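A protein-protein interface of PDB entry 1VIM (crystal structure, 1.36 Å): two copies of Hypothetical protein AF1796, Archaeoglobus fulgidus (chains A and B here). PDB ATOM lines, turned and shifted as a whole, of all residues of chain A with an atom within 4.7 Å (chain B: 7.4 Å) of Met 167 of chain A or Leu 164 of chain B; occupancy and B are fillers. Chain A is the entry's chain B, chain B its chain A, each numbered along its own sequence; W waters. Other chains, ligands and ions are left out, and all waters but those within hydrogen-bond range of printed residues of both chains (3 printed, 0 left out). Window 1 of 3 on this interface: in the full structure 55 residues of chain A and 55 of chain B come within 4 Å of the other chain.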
ATOM      1  N   ILE A  61      -7.751 -26.242 -38.537  1.00  0.00           N
ATOM      2  CA  ILE A  61      -8.544 -27.331 -37.945  1.00  0.00           C
ATOM      3  C   ILE A  61      -7.860 -28.659 -38.215  1.00  0.00           C
ATOM      4  O   ILE A  61      -7.715 -29.500 -37.315  1.00  0.00           O
ATOM      5  CB  ILE A  61      -9.978 -27.318 -38.477  1.00  0.00           C
ATOM      6  CG1 ILE A  61     -10.649 -26.026 -38.031  1.00  0.00           C
ATOM      7  CG2 ILE A  61     -10.749 -28.524 -37.942  1.00  0.00           C
ATOM      8  CD1 ILE A  61     -11.944 -25.790 -38.691  1.00  0.00           C
ATOM      9  N   ALA A  64      -4.882 -28.986 -35.920  1.00  0.00           N
ATOM     10  CA  ALA A  64      -5.293 -29.298 -34.551  1.00  0.00           C
ATOM     11  C   ALA A  64      -5.651 -30.776 -34.428  1.00  0.00           C
ATOM     12  O   ALA A  64      -5.272 -31.427 -33.437  1.00  0.00           O
ATOM     13  CB  ALA A  64      -6.501 -28.452 -34.158  1.00  0.00           C
ATOM     14  N   PHE A  65      -6.367 -31.308 -35.418  1.00  0.00           N
ATOM     15  CA  PHE A  65      -6.759 -32.722 -35.400  1.00  0.00           C
ATOM     16  C   PHE A  65      -5.531 -33.642 -35.565  1.00  0.00           C
ATOM     17  O   PHE A  65      -5.390 -34.629 -34.814  1.00  0.00           O
ATOM     18  CB  PHE A  65      -7.769 -32.955 -36.514  1.00  0.00           C
ATOM     19  CG  PHE A  65      -8.310 -34.370 -36.596  1.00  0.00           C
ATOM     20  CD1 PHE A  65      -8.805 -35.024 -35.459  1.00  0.00           C
ATOM     21  CD2 PHE A  65      -8.319 -35.038 -37.813  1.00  0.00           C
ATOM     22  CE1 PHE A  65      -9.311 -36.330 -35.567  1.00  0.00           C
ATOM     23  CE2 PHE A  65      -8.860 -36.335 -37.919  1.00  0.00           C
ATOM     24  CZ  PHE A  65      -9.336 -36.973 -36.799  1.00  0.00           C
ATOM     25  N   GLU A 163     -16.593 -24.297 -39.733  1.00  0.00           N
ATOM     26  CA  GLU A 163     -15.303 -24.458 -39.082  1.00  0.00           C
ATOM     27  C   GLU A 163     -15.414 -24.784 -37.599  1.00  0.00           C
ATOM     28  O   GLU A 163     -14.790 -25.739 -37.148  1.00  0.00           O
ATOM     29  CB  GLU A 163     -14.453 -23.224 -39.333  1.00  0.00           C
ATOM     30  CG  GLU A 163     -14.108 -23.084 -40.806  1.00  0.00           C
ATOM     31  CD  GLU A 163     -13.749 -21.686 -41.200  1.00  0.00           C
ATOM     32  OE1 GLU A 163     -13.694 -20.818 -40.313  1.00  0.00           O
ATOM     33  OE2 GLU A 163     -13.548 -21.467 -42.405  1.00  0.00           O
ATOM     34  N   LEU A 164     -16.271 -24.071 -36.865  1.00  0.00           N
ATOM     35  CA  LEU A 164     -16.437 -24.346 -35.432  1.00  0.00           C
ATOM     36  C   LEU A 164     -17.042 -25.725 -35.245  1.00  0.00           C
ATOM     37  O   LEU A 164     -16.641 -26.477 -34.366  1.00  0.00           O
ATOM     38  CB  LEU A 164     -17.357 -23.312 -34.790  1.00  0.00           C
ATOM     39  CG  LEU A 164     -16.822 -21.910 -34.618  1.00  0.00           C
ATOM     40  CD1 LEU A 164     -17.992 -21.040 -34.154  1.00  0.00           C
ATOM     41  CD2 LEU A 164     -15.660 -21.933 -33.628  1.00  0.00           C
ATOM     42  N   THR A 165     -18.012 -26.062 -36.092  1.00  0.00           N
ATOM     43  CA  THR A 165     -18.693 -27.348 -35.949  1.00  0.00           C
ATOM     44  C   THR A 165     -17.724 -28.490 -36.251  1.00  0.00           C
ATOM     45  O   THR A 165     -17.709 -29.481 -35.516  1.00  0.00           O
ATOM     46  CB  THR A 165     -19.938 -27.416 -36.830  1.00  0.00           C
ATOM     47  OG1 THR A 165     -20.768 -26.280 -36.535  1.00  0.00           O
ATOM     48  CG2 THR A 165     -20.809 -28.643 -36.433  1.00  0.00           C
ATOM     49  N   ALA A 166     -16.902 -28.331 -37.288  1.00  0.00           N
ATOM     50  CA  ALA A 166     -15.919 -29.361 -37.632  1.00  0.00           C
ATOM     51  C   ALA A 166     -14.887 -29.518 -36.512  1.00  0.00           C
ATOM     52  O   ALA A 166     -14.538 -30.649 -36.170  1.00  0.00           O
ATOM     53  CB  ALA A 166     -15.221 -29.047 -38.992  1.00  0.00           C
ATOM     54  N   MET A 167     -14.426 -28.414 -35.924  1.00  0.00           N
ATOM     55  CA  MET A 167     -13.470 -28.492 -34.830  1.00  0.00           C
ATOM     56  C   MET A 167     -14.055 -29.237 -33.645  1.00  0.00           C
ATOM     57  O   MET A 167     -13.423 -30.152 -33.099  1.00  0.00           O
ATOM     58  CB  MET A 167     -13.035 -27.086 -34.430  1.00  0.00           C
ATOM     59  CG  MET A 167     -11.783 -27.149 -33.480  1.00  0.00           C
ATOM     60  SD  MET A 167     -10.241 -27.905 -34.120  1.00  0.00           S
ATOM     61  CE  MET A 167     -10.389 -29.769 -33.752  1.00  0.00           C
ATOM     62  N   ILE A 168     -15.312 -28.916 -33.324  1.00  0.00           N
ATOM     63  CA  ILE A 168     -16.004 -29.562 -32.197  1.00  0.00           C
ATOM     64  C   ILE A 168     -16.218 -31.056 -32.483  1.00  0.00           C
ATOM     65  O   ILE A 168     -15.940 -31.926 -31.620  1.00  0.00           O
ATOM     66  CB  ILE A 168     -17.319 -28.822 -31.884  1.00  0.00           C
ATOM     67  CG1 ILE A 168     -17.006 -27.484 -31.215  1.00  0.00           C
ATOM     68  CG2 ILE A 168     -18.218 -29.665 -30.966  1.00  0.00           C
ATOM     69  CD1 ILE A 168     -18.151 -26.488 -31.253  1.00  0.00           C
ATOM     70  N   PHE A 169     -16.641 -31.376 -33.711  1.00  0.00           N
ATOM     71  CA  PHE A 169     -16.831 -32.768 -34.079  1.00  0.00           C
ATOM     72  C   PHE A 169     -15.498 -33.548 -33.978  1.00  0.00           C
ATOM     73  O   PHE A 169     -15.481 -34.675 -33.470  1.00  0.00           O
ATOM     74  CB  PHE A 169     -17.384 -32.900 -35.495  1.00  0.00           C
ATOM     75  CG  PHE A 169     -17.277 -34.277 -36.025  1.00  0.00           C
ATOM     76  CD1 PHE A 169     -18.120 -35.265 -35.537  1.00  0.00           C
ATOM     77  CD2 PHE A 169     -16.287 -34.607 -36.919  1.00  0.00           C
ATOM     78  CE1 PHE A 169     -17.981 -36.594 -35.992  1.00  0.00           C
ATOM     79  CE2 PHE A 169     -16.147 -35.928 -37.376  1.00  0.00           C
ATOM     80  CZ  PHE A 169     -17.003 -36.910 -36.902  1.00  0.00           C
ATOM     81  N   LEU A 170     -14.409 -32.989 -34.504  1.00  0.00           N
ATOM     82  CA  LEU A 170     -13.130 -33.723 -34.485  1.00  0.00           C
ATOM     83  C   LEU A 170     -12.624 -33.919 -33.055  1.00  0.00           C
ATOM     84  O   LEU A 170     -12.079 -34.983 -32.757  1.00  0.00           O
ATOM     85  CB  LEU A 170     -12.088 -33.039 -35.373  1.00  0.00           C
ATOM     86  CG  LEU A 170     -12.500 -33.134 -36.853  1.00  0.00           C
ATOM     87  CD1 LEU A 170     -11.635 -32.154 -37.671  1.00  0.00           C
ATOM     88  CD2 LEU A 170     -12.317 -34.556 -37.383  1.00  0.00           C
ATOM     89  N   ASP A 171     -12.818 -32.940 -32.162  1.00  0.00           N
ATOM     90  CA  ASP A 171     -12.505 -33.169 -30.746  1.00  0.00           C
ATOM     91  C   ASP A 171     -13.424 -34.201 -30.090  1.00  0.00           C
ATOM     92  O   ASP A 171     -12.994 -34.985 -29.233  1.00  0.00           O
ATOM     93  CB  ASP A 171     -12.521 -31.841 -29.988  1.00  0.00           C
ATOM     94  CG  ASP A 171     -11.250 -31.019 -30.209  1.00  0.00           C
ATOM     95  OD1 ASP A 171     -10.143 -31.570 -30.398  1.00  0.00           O
ATOM     96  OD2 ASP A 171     -11.313 -29.790 -30.178  1.00  0.00           O
ATOM     97  N   PHE B  17     -19.087 -35.863 -24.944  1.00  0.00           N
ATOM     98  CA  PHE B  17     -18.239 -34.715 -25.189  1.00  0.00           C
ATOM     99  C   PHE B  17     -19.061 -33.527 -25.741  1.00  0.00           C
ATOM    100  O   PHE B  17     -18.900 -32.397 -25.302  1.00  0.00           O
ATOM    101  CB  PHE B  17     -17.117 -35.105 -26.173  1.00  0.00           C
ATOM    102  CG  PHE B  17     -16.225 -33.945 -26.536  1.00  0.00           C
ATOM    103  CD1 PHE B  17     -16.530 -33.154 -27.646  1.00  0.00           C
ATOM    104  CD2 PHE B  17     -15.125 -33.608 -25.761  1.00  0.00           C
ATOM    105  CE1 PHE B  17     -15.740 -32.073 -27.975  1.00  0.00           C
ATOM    106  CE2 PHE B  17     -14.322 -32.528 -26.103  1.00  0.00           C
ATOM    107  CZ  PHE B  17     -14.646 -31.746 -27.214  1.00  0.00           C
ATOM    108  N   VAL B  21     -19.492 -29.698 -24.301  1.00  0.00           N
ATOM    109  CA  VAL B  21     -19.280 -28.480 -25.082  1.00  0.00           C
ATOM    110  C   VAL B  21     -20.510 -27.557 -24.974  1.00  0.00           C
ATOM    111  O   VAL B  21     -20.341 -26.361 -24.726  1.00  0.00           O
ATOM    112  CB  VAL B  21     -18.955 -28.809 -26.560  1.00  0.00           C
ATOM    113  CG1 VAL B  21     -18.909 -27.526 -27.422  1.00  0.00           C
ATOM    114  CG2 VAL B  21     -17.606 -29.483 -26.619  1.00  0.00           C
ATOM    115  N   ILE B  25     -20.519 -23.691 -23.546  1.00  0.00           N
ATOM    116  CA  ILE B  25     -20.906 -22.504 -24.305  1.00  0.00           C
ATOM    117  C   ILE B  25     -22.006 -21.751 -23.558  1.00  0.00           C
ATOM    118  O   ILE B  25     -21.970 -20.522 -23.490  1.00  0.00           O
ATOM    119  CB  ILE B  25     -21.364 -22.846 -25.728  1.00  0.00           C
ATOM    120  CG1 ILE B  25     -20.314 -23.640 -26.499  1.00  0.00           C
ATOM    121  CG2 ILE B  25     -21.702 -21.554 -26.501  1.00  0.00           C
ATOM    122  CD1 ILE B  25     -20.959 -24.448 -27.717  1.00  0.00           C
ATOM    123  N   LEU B  28     -20.264 -19.810 -20.869  1.00  0.00           N
ATOM    124  CA  LEU B  28     -19.663 -18.606 -21.408  1.00  0.00           C
ATOM    125  C   LEU B  28     -20.702 -17.519 -21.624  1.00  0.00           C
ATOM    126  O   LEU B  28     -20.473 -16.369 -21.255  1.00  0.00           O
ATOM    127  CB  LEU B  28     -18.948 -18.933 -22.710  1.00  0.00           C
ATOM    128  CG  LEU B  28     -18.294 -17.786 -23.469  1.00  0.00           C
ATOM    129  CD1 LEU B  28     -17.145 -17.193 -22.663  1.00  0.00           C
ATOM    130  CD2 LEU B  28     -17.808 -18.279 -24.823  1.00  0.00           C
ATOM    131  N   ARG B  57      -1.814 -25.897 -30.403  1.00  0.00           N
ATOM    132  CA  ARG B  57      -3.204 -25.680 -30.800  1.00  0.00           C
ATOM    133  C   ARG B  57      -3.713 -24.266 -30.519  1.00  0.00           C
ATOM    134  O   ARG B  57      -4.490 -23.722 -31.316  1.00  0.00           O
ATOM    135  CB  ARG B  57      -4.113 -26.754 -30.213  1.00  0.00           C
ATOM    136  CG  ARG B  57      -4.067 -28.036 -31.062  1.00  0.00           C
ATOM    137  CD  ARG B  57      -4.605 -29.288 -30.400  1.00  0.00           C
ATOM    138  NE  ARG B  57      -5.951 -29.078 -29.901  1.00  0.00           N
ATOM    139  CZ  ARG B  57      -7.033 -29.788 -30.243  1.00  0.00           C
ATOM    140  NH1 ARG B  57      -6.988 -30.727 -31.187  1.00  0.00           N
ATOM    141  NH2 ARG B  57      -8.190 -29.509 -29.652  1.00  0.00           N
ATOM    142  N   TYR B  60      -2.935 -22.204 -33.458  1.00  0.00           N
ATOM    143  CA  TYR B  60      -3.885 -22.340 -34.554  1.00  0.00           C
ATOM    144  C   TYR B  60      -5.112 -21.472 -34.331  1.00  0.00           C
ATOM    145  O   TYR B  60      -5.649 -20.902 -35.293  1.00  0.00           O
ATOM    146  CB  TYR B  60      -4.284 -23.809 -34.796  1.00  0.00           C
ATOM    147  CG  TYR B  60      -3.104 -24.751 -34.907  1.00  0.00           C
ATOM    148  CD1 TYR B  60      -1.886 -24.343 -35.479  1.00  0.00           C
ATOM    149  CD2 TYR B  60      -3.206 -26.042 -34.397  1.00  0.00           C
ATOM    150  CE1 TYR B  60      -0.797 -25.237 -35.537  1.00  0.00           C
ATOM    151  CE2 TYR B  60      -2.125 -26.926 -34.430  1.00  0.00           C
ATOM    152  CZ  TYR B  60      -0.951 -26.514 -35.003  1.00  0.00           C
ATOM    153  OH  TYR B  60       0.112 -27.382 -34.992  1.00  0.00           O
ATOM    154  N   ILE B  61      -5.537 -21.334 -33.074  1.00  0.00           N
ATOM    155  CA  ILE B  61      -6.637 -20.433 -32.749  1.00  0.00           C
ATOM    156  C   ILE B  61      -6.217 -18.981 -32.996  1.00  0.00           C
ATOM    157  O   ILE B  61      -6.981 -18.189 -33.562  1.00  0.00           O
ATOM    158  CB  ILE B  61      -7.027 -20.621 -31.268  1.00  0.00           C
ATOM    159  CG1 ILE B  61      -7.500 -22.045 -30.996  1.00  0.00           C
ATOM    160  CG2 ILE B  61      -8.047 -19.560 -30.839  1.00  0.00           C
ATOM    161  CD1 ILE B  61      -7.734 -22.312 -29.585  1.00  0.00           C
ATOM    162  N   VAL B 140     -11.461 -16.673 -20.297  1.00  0.00           N
ATOM    163  CA  VAL B 140     -12.267 -17.679 -20.960  1.00  0.00           C
ATOM    164  C   VAL B 140     -11.856 -18.984 -20.323  1.00  0.00           C
ATOM    165  O   VAL B 140     -10.742 -19.441 -20.525  1.00  0.00           O
ATOM    166  CB  VAL B 140     -12.003 -17.708 -22.500  1.00  0.00           C
ATOM    167  CG1 VAL B 140     -12.840 -18.751 -23.154  1.00  0.00           C
ATOM    168  CG2 VAL B 140     -12.302 -16.306 -23.123  1.00  0.00           C
ATOM    169  N   LYS B 141     -12.730 -19.553 -19.501  1.00  0.00           N
ATOM    170  CA  LYS B 141     -12.387 -20.782 -18.744  1.00  0.00           C
ATOM    171  C   LYS B 141     -12.355 -22.018 -19.603  1.00  0.00           C
ATOM    172  O   LYS B 141     -13.151 -22.153 -20.529  1.00  0.00           O
ATOM    173  CB  LYS B 141     -13.447 -21.067 -17.676  1.00  0.00           C
ATOM    174  CG  LYS B 141     -13.750 -19.933 -16.753  1.00  0.00           C
ATOM    175  CD  LYS B 141     -12.524 -19.572 -15.927  1.00  0.00           C
ATOM    176  CE  LYS B 141     -12.263 -20.582 -14.828  1.00  0.00           C
ATOM    177  NZ  LYS B 141     -10.831 -20.590 -14.387  1.00  0.00           N
ATOM    178  N   ALA B 156     -11.868 -34.243 -22.689  1.00  0.00           N
ATOM    179  CA  ALA B 156     -11.319 -32.999 -23.262  1.00  0.00           C
ATOM    180  C   ALA B 156      -9.898 -32.843 -22.736  1.00  0.00           C
ATOM    181  O   ALA B 156      -9.634 -32.042 -21.838  1.00  0.00           O
ATOM    182  CB  ALA B 156     -12.194 -31.815 -22.875  1.00  0.00           C
ATOM    183  N   GLY B 159      -6.321 -29.424 -22.235  1.00  0.00           N
ATOM    184  CA  GLY B 159      -6.813 -28.065 -22.490  1.00  0.00           C
ATOM    185  C   GLY B 159      -7.745 -27.892 -23.697  1.00  0.00           C
ATOM    186  O   GLY B 159      -8.044 -26.759 -24.090  1.00  0.00           O
ATOM    187  N   THR B 160      -8.242 -28.990 -24.254  1.00  0.00           N
ATOM    188  CA  THR B 160      -9.220 -28.951 -25.346  1.00  0.00           C
ATOM    189  C   THR B 160     -10.397 -28.036 -25.070  1.00  0.00           C
ATOM    190  O   THR B 160     -10.830 -27.312 -25.959  1.00  0.00           O
ATOM    191  CB  THR B 160      -9.744 -30.391 -25.574  1.00  0.00           C
ATOM    192  OG1 THR B 160      -8.710 -31.190 -26.176  1.00  0.00           O
ATOM    193  CG2 THR B 160     -10.899 -30.438 -26.581  1.00  0.00           C
ATOM    194  N   MET B 161     -10.963 -28.107 -23.874  1.00  0.00           N
ATOM    195  CA  MET B 161     -12.134 -27.274 -23.620  1.00  0.00           C
ATOM    196  C   MET B 161     -11.817 -25.785 -23.637  1.00  0.00           C
ATOM    197  O   MET B 161     -12.588 -25.012 -24.192  1.00  0.00           O
ATOM    198  CB  MET B 161     -12.828 -27.663 -22.323  1.00  0.00           C
ATOM    199  CG  MET B 161     -14.279 -27.199 -22.235  1.00  0.00           C
ATOM    200  SD  MET B 161     -15.366 -27.737 -23.605  1.00  0.00           S
ATOM    201  CE  MET B 161     -14.821 -29.488 -23.712  1.00  0.00           C
ATOM    202  N   PHE B 162     -10.690 -25.383 -23.059  1.00  0.00           N
ATOM    203  CA  PHE B 162     -10.266 -23.990 -23.182  1.00  0.00           C
ATOM    204  C   PHE B 162     -10.142 -23.618 -24.671  1.00  0.00           C
ATOM    205  O   PHE B 162     -10.595 -22.546 -25.106  1.00  0.00           O
ATOM    206  CB  PHE B 162      -8.905 -23.725 -22.510  1.00  0.00           C
ATOM    207  CG  PHE B 162      -8.321 -22.403 -22.911  1.00  0.00           C
ATOM    208  CD1 PHE B 162      -8.824 -21.228 -22.342  1.00  0.00           C
ATOM    209  CD2 PHE B 162      -7.337 -22.323 -23.912  1.00  0.00           C
ATOM    210  CE1 PHE B 162      -8.341 -19.974 -22.746  1.00  0.00           C
ATOM    211  CE2 PHE B 162      -6.861 -21.084 -24.327  1.00  0.00           C
ATOM    212  CZ  PHE B 162      -7.351 -19.909 -23.746  1.00  0.00           C
ATOM    213  N   GLU B 163      -9.517 -24.476 -25.468  1.00  0.00           N
ATOM    214  CA  GLU B 163      -9.237 -24.117 -26.858  1.00  0.00           C
ATOM    215  C   GLU B 163     -10.524 -23.937 -27.647  1.00  0.00           C
ATOM    216  O   GLU B 163     -10.693 -22.945 -28.339  1.00  0.00           O
ATOM    217  CB  GLU B 163      -8.367 -25.188 -27.505  1.00  0.00           C
ATOM    218  CG  GLU B 163      -7.000 -25.257 -26.842  1.00  0.00           C
ATOM    219  CD  GLU B 163      -6.220 -26.459 -27.216  1.00  0.00           C
ATOM    220  OE1 GLU B 163      -6.753 -27.313 -27.943  1.00  0.00           O
ATOM    221  OE2 GLU B 163      -5.069 -26.542 -26.721  1.00  0.00           O
ATOM    222  N   LEU B 164     -11.475 -24.853 -27.485  1.00  0.00           N
ATOM    223  CA  LEU B 164     -12.754 -24.699 -28.185  1.00  0.00           C
ATOM    224  C   LEU B 164     -13.502 -23.465 -27.712  1.00  0.00           C
ATOM    225  O   LEU B 164     -14.082 -22.735 -28.508  1.00  0.00           O
ATOM    226  CB  LEU B 164     -13.637 -25.941 -27.941  1.00  0.00           C
ATOM    227  CG  LEU B 164     -13.163 -27.213 -28.595  1.00  0.00           C
ATOM    228  CD1 LEU B 164     -14.074 -28.348 -28.172  1.00  0.00           C
ATOM    229  CD2 LEU B 164     -13.103 -27.044 -30.114  1.00  0.00           C
ATOM    230  N   THR B 165     -13.483 -23.223 -26.418  1.00  0.00           N
ATOM    231  CA  THR B 165     -14.240 -22.100 -25.895  1.00  0.00           C
ATOM    232  C   THR B 165     -13.601 -20.785 -26.351  1.00  0.00           C
ATOM    233  O   THR B 165     -14.307 -19.829 -26.686  1.00  0.00           O
ATOM    234  CB  THR B 165     -14.299 -22.177 -24.362  1.00  0.00           C
ATOM    235  OG1 THR B 165     -14.857 -23.442 -23.973  1.00  0.00           O
ATOM    236  CG2 THR B 165     -15.284 -21.133 -23.793  1.00  0.00           C
ATOM    237  N   ALA B 166     -12.273 -20.732 -26.366  1.00  0.00           N
ATOM    238  CA  ALA B 166     -11.565 -19.541 -26.813  1.00  0.00           C
ATOM    239  C   ALA B 166     -11.832 -19.284 -28.304  1.00  0.00           C
ATOM    240  O   ALA B 166     -12.060 -18.142 -28.715  1.00  0.00           O
ATOM    241  CB  ALA B 166     -10.049 -19.666 -26.520  1.00  0.00           C
ATOM    242  N   MET B 167     -11.845 -20.338 -29.115  1.00  0.00           N
ATOM    243  CA  MET B 167     -12.156 -20.183 -30.525  1.00  0.00           C
ATOM    244  C   MET B 167     -13.552 -19.610 -30.695  1.00  0.00           C
ATOM    245  O   MET B 167     -13.762 -18.661 -31.481  1.00  0.00           O
ATOM    246  CB  MET B 167     -12.044 -21.526 -31.259  1.00  0.00           C
ATOM    247  CG  MET B 167     -12.123 -21.374 -32.789  1.00  0.00           C
ATOM    248  SD  MET B 167     -10.779 -20.368 -33.620  1.00  0.00           S
ATOM    249  CE  MET B 167     -11.448 -18.612 -33.704  1.00  0.00           C
ATOM    250  N   ILE B 168     -14.515 -20.158 -29.965  1.00  0.00           N
ATOM    251  CA  ILE B 168     -15.896 -19.705 -30.097  1.00  0.00           C
ATOM    252  C   ILE B 168     -16.021 -18.255 -29.618  1.00  0.00           C
ATOM    253  O   ILE B 168     -16.671 -17.420 -30.268  1.00  0.00           O
ATOM    254  CB  ILE B 168     -16.815 -20.645 -29.283  1.00  0.00           C
ATOM    255  CG1 ILE B 168     -16.949 -21.979 -30.011  1.00  0.00           C
ATOM    256  CG2 ILE B 168     -18.197 -20.009 -29.096  1.00  0.00           C
ATOM    257  CD1 ILE B 168     -17.458 -23.112 -29.132  1.00  0.00           C
ATOM    258  N   PHE B 169     -15.373 -17.928 -28.495  1.00  0.00           N
ATOM    259  CA  PHE B 169     -15.322 -16.557 -28.026  1.00  0.00           C
ATOM    260  C   PHE B 169     -14.759 -15.594 -29.071  1.00  0.00           C
ATOM    261  O   PHE B 169     -15.306 -14.505 -29.297  1.00  0.00           O
ATOM    262  CB  PHE B 169     -14.518 -16.421 -26.725  1.00  0.00           C
ATOM    263  CG  PHE B 169     -14.184 -15.006 -26.410  1.00  0.00           C
ATOM    264  CD1 PHE B 169     -15.189 -14.114 -26.024  1.00  0.00           C
ATOM    265  CD2 PHE B 169     -12.897 -14.534 -26.611  1.00  0.00           C
ATOM    266  CE1 PHE B 169     -14.867 -12.785 -25.804  1.00  0.00           C
ATOM    267  CE2 PHE B 169     -12.575 -13.218 -26.369  1.00  0.00           C
ATOM    268  CZ  PHE B 169     -13.561 -12.340 -25.977  1.00  0.00           C
ATOM    269  N   LEU B 170     -13.629 -15.956 -29.680  1.00  0.00           N
ATOM    270  CA  LEU B 170     -12.993 -15.041 -30.656  1.00  0.00           C
ATOM    271  C   LEU B 170     -13.885 -14.849 -31.889  1.00  0.00           C
ATOM    272  O   LEU B 170     -13.942 -13.745 -32.449  1.00  0.00           O
ATOM    273  CB  LEU B 170     -11.594 -15.534 -31.007  1.00  0.00           C
ATOM    274  CG  LEU B 170     -10.642 -15.392 -29.806  1.00  0.00           C
ATOM    275  CD1 LEU B 170      -9.331 -16.161 -30.033  1.00  0.00           C
ATOM    276  CD2 LEU B 170     -10.348 -13.947 -29.489  1.00  0.00           C
ATOM    277  N   ASP B 171     -14.595 -15.902 -32.304  1.00  0.00           N
ATOM    278  CA  ASP B 171     -15.549 -15.739 -33.405  1.00  0.00           C
ATOM    279  C   ASP B 171     -16.749 -14.884 -32.972  1.00  0.00           C
ATOM    280  O   ASP B 171     -17.265 -14.080 -33.768  1.00  0.00           O
ATOM    281  CB  ASP B 171     -16.060 -17.073 -33.925  1.00  0.00           C
ATOM    282  CG  ASP B 171     -15.067 -17.791 -34.766  1.00  0.00           C
ATOM    283  OD1 ASP B 171     -14.274 -17.155 -35.484  1.00  0.00           O
ATOM    284  OD2 ASP B 171     -15.054 -19.037 -34.771  1.00  0.00           O
HETATM  285  O   HOH W   1     -10.222 -27.860 -28.918  1.00  0.00           O
HETATM  286  O   HOH W   2      -9.127 -33.255 -28.350  1.00  0.00           O
HETATM  287  O   HOH W   3      -9.044 -32.562 -32.751  1.00  0.00           O
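NH1 of Arg 57 of chain B sits at hydrogen-bond distance from O of Ala 64 of chain A (2.9 Å).
The guanidinium group (NH2) of Arg 57 of chain B lies within salt-bridge range of the side-chain carboxylate (OD1) of Asp 171 of chain A (2.9 Å).
Leu 164 of chain A touches Met 167 of chain B, and with the chains exchanged Met 167 of chain A touches Leu 164 of chain B.
Leu 164 of chain A touches Ile 168 of chain B, but with the chains exchanged Ile 168 of chain A does not touch Leu 164 of chain B (4.1 Å).
Leu 164 of chain A touches Asp 171 of chain B, and with the chains exchanged Asp 171 of chain A touches Leu 164 of chain B.
10 positions are printed for both chains.
No residue of chain B comes within 4 Å of Ala 166 of chain A.
Printed residues of chain B within 4 Å of Met 167 of chain A: Leu 164 (3.6 Å).
Of the printed residues of chain B, Ile 168 of chain A touches Phe 17.
Of the printed residues of chain B, Asp 171 of chain A touches Phe 17, Arg 57, Thr 160 and Leu 164.
Of the printed residues of chain A, Tyr 60 of chain B touches Ala 64.
Val 140 of chain B touches none of the printed residues of chain A.
The nearest printed residue of chain B that does not touch Met 167 of chain A is Arg 57 of chain B (4.4 Å).
Among the printed residues, merely in contact across the chains: Ala 64 of chain A with Tyr 60 of chain B (3.7 Å), Leu 164 of chain A with Met 167 of chain B (3.7 Å), Leu 164 of chain A with Ile 168 of chain B (3.8 Å), Leu 164 of chain A with Asp 171 of chain B (3.2 Å), Met 167 of chain A with Leu 164 of chain B (3.6 Å), Ile 168 of chain A with Phe 17 of chain B (3.7 Å), Asp 171 of chain A with Phe 17 of chain B (3.5 Å), Asp 171 of chain A with Thr 160 of chain B (3.7 Å) and Asp 171 of chain A with Leu 164 of chain B (3.3 Å).
Of the 23 printed residues of chain B, 8 touch a printed residue of chain A.
Hydrophobic or aromatic side chains of chain B that line the printed part of chain A: Phe 17, Tyr 60, Leu 164, Met 167 and Ile 168.
Of the 12 printed residues of chain A, 5 touch a printed residue of chain B.
Among the printed residues, 11 pairs touch across the chains.
OE1 of Glu 163 of chain B is in salt-bridge range of NE of Arg 57 of chain B (2.8 Å).
Water W1 lies within hydrogen-bond range of the side-chain carboxylate of Asp 171 of chain A (2.6 Å), the guanidinium group of Arg 57 of chain B (2.7 Å) and the backbone carbonyl oxygen of Thr 160 of chain B (3.1 Å).
Water W3 lies within hydrogen-bond range of OD1 of Asp 171 of chain A (2.8 Å) and NH1 of Arg 57 of chain B (3.2 Å).
Water W2 lies within hydrogen-bond range of OD1 of Asp 171 of chain A (2.8 Å) and OG1 of Thr 160 of chain B (3.0 Å).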
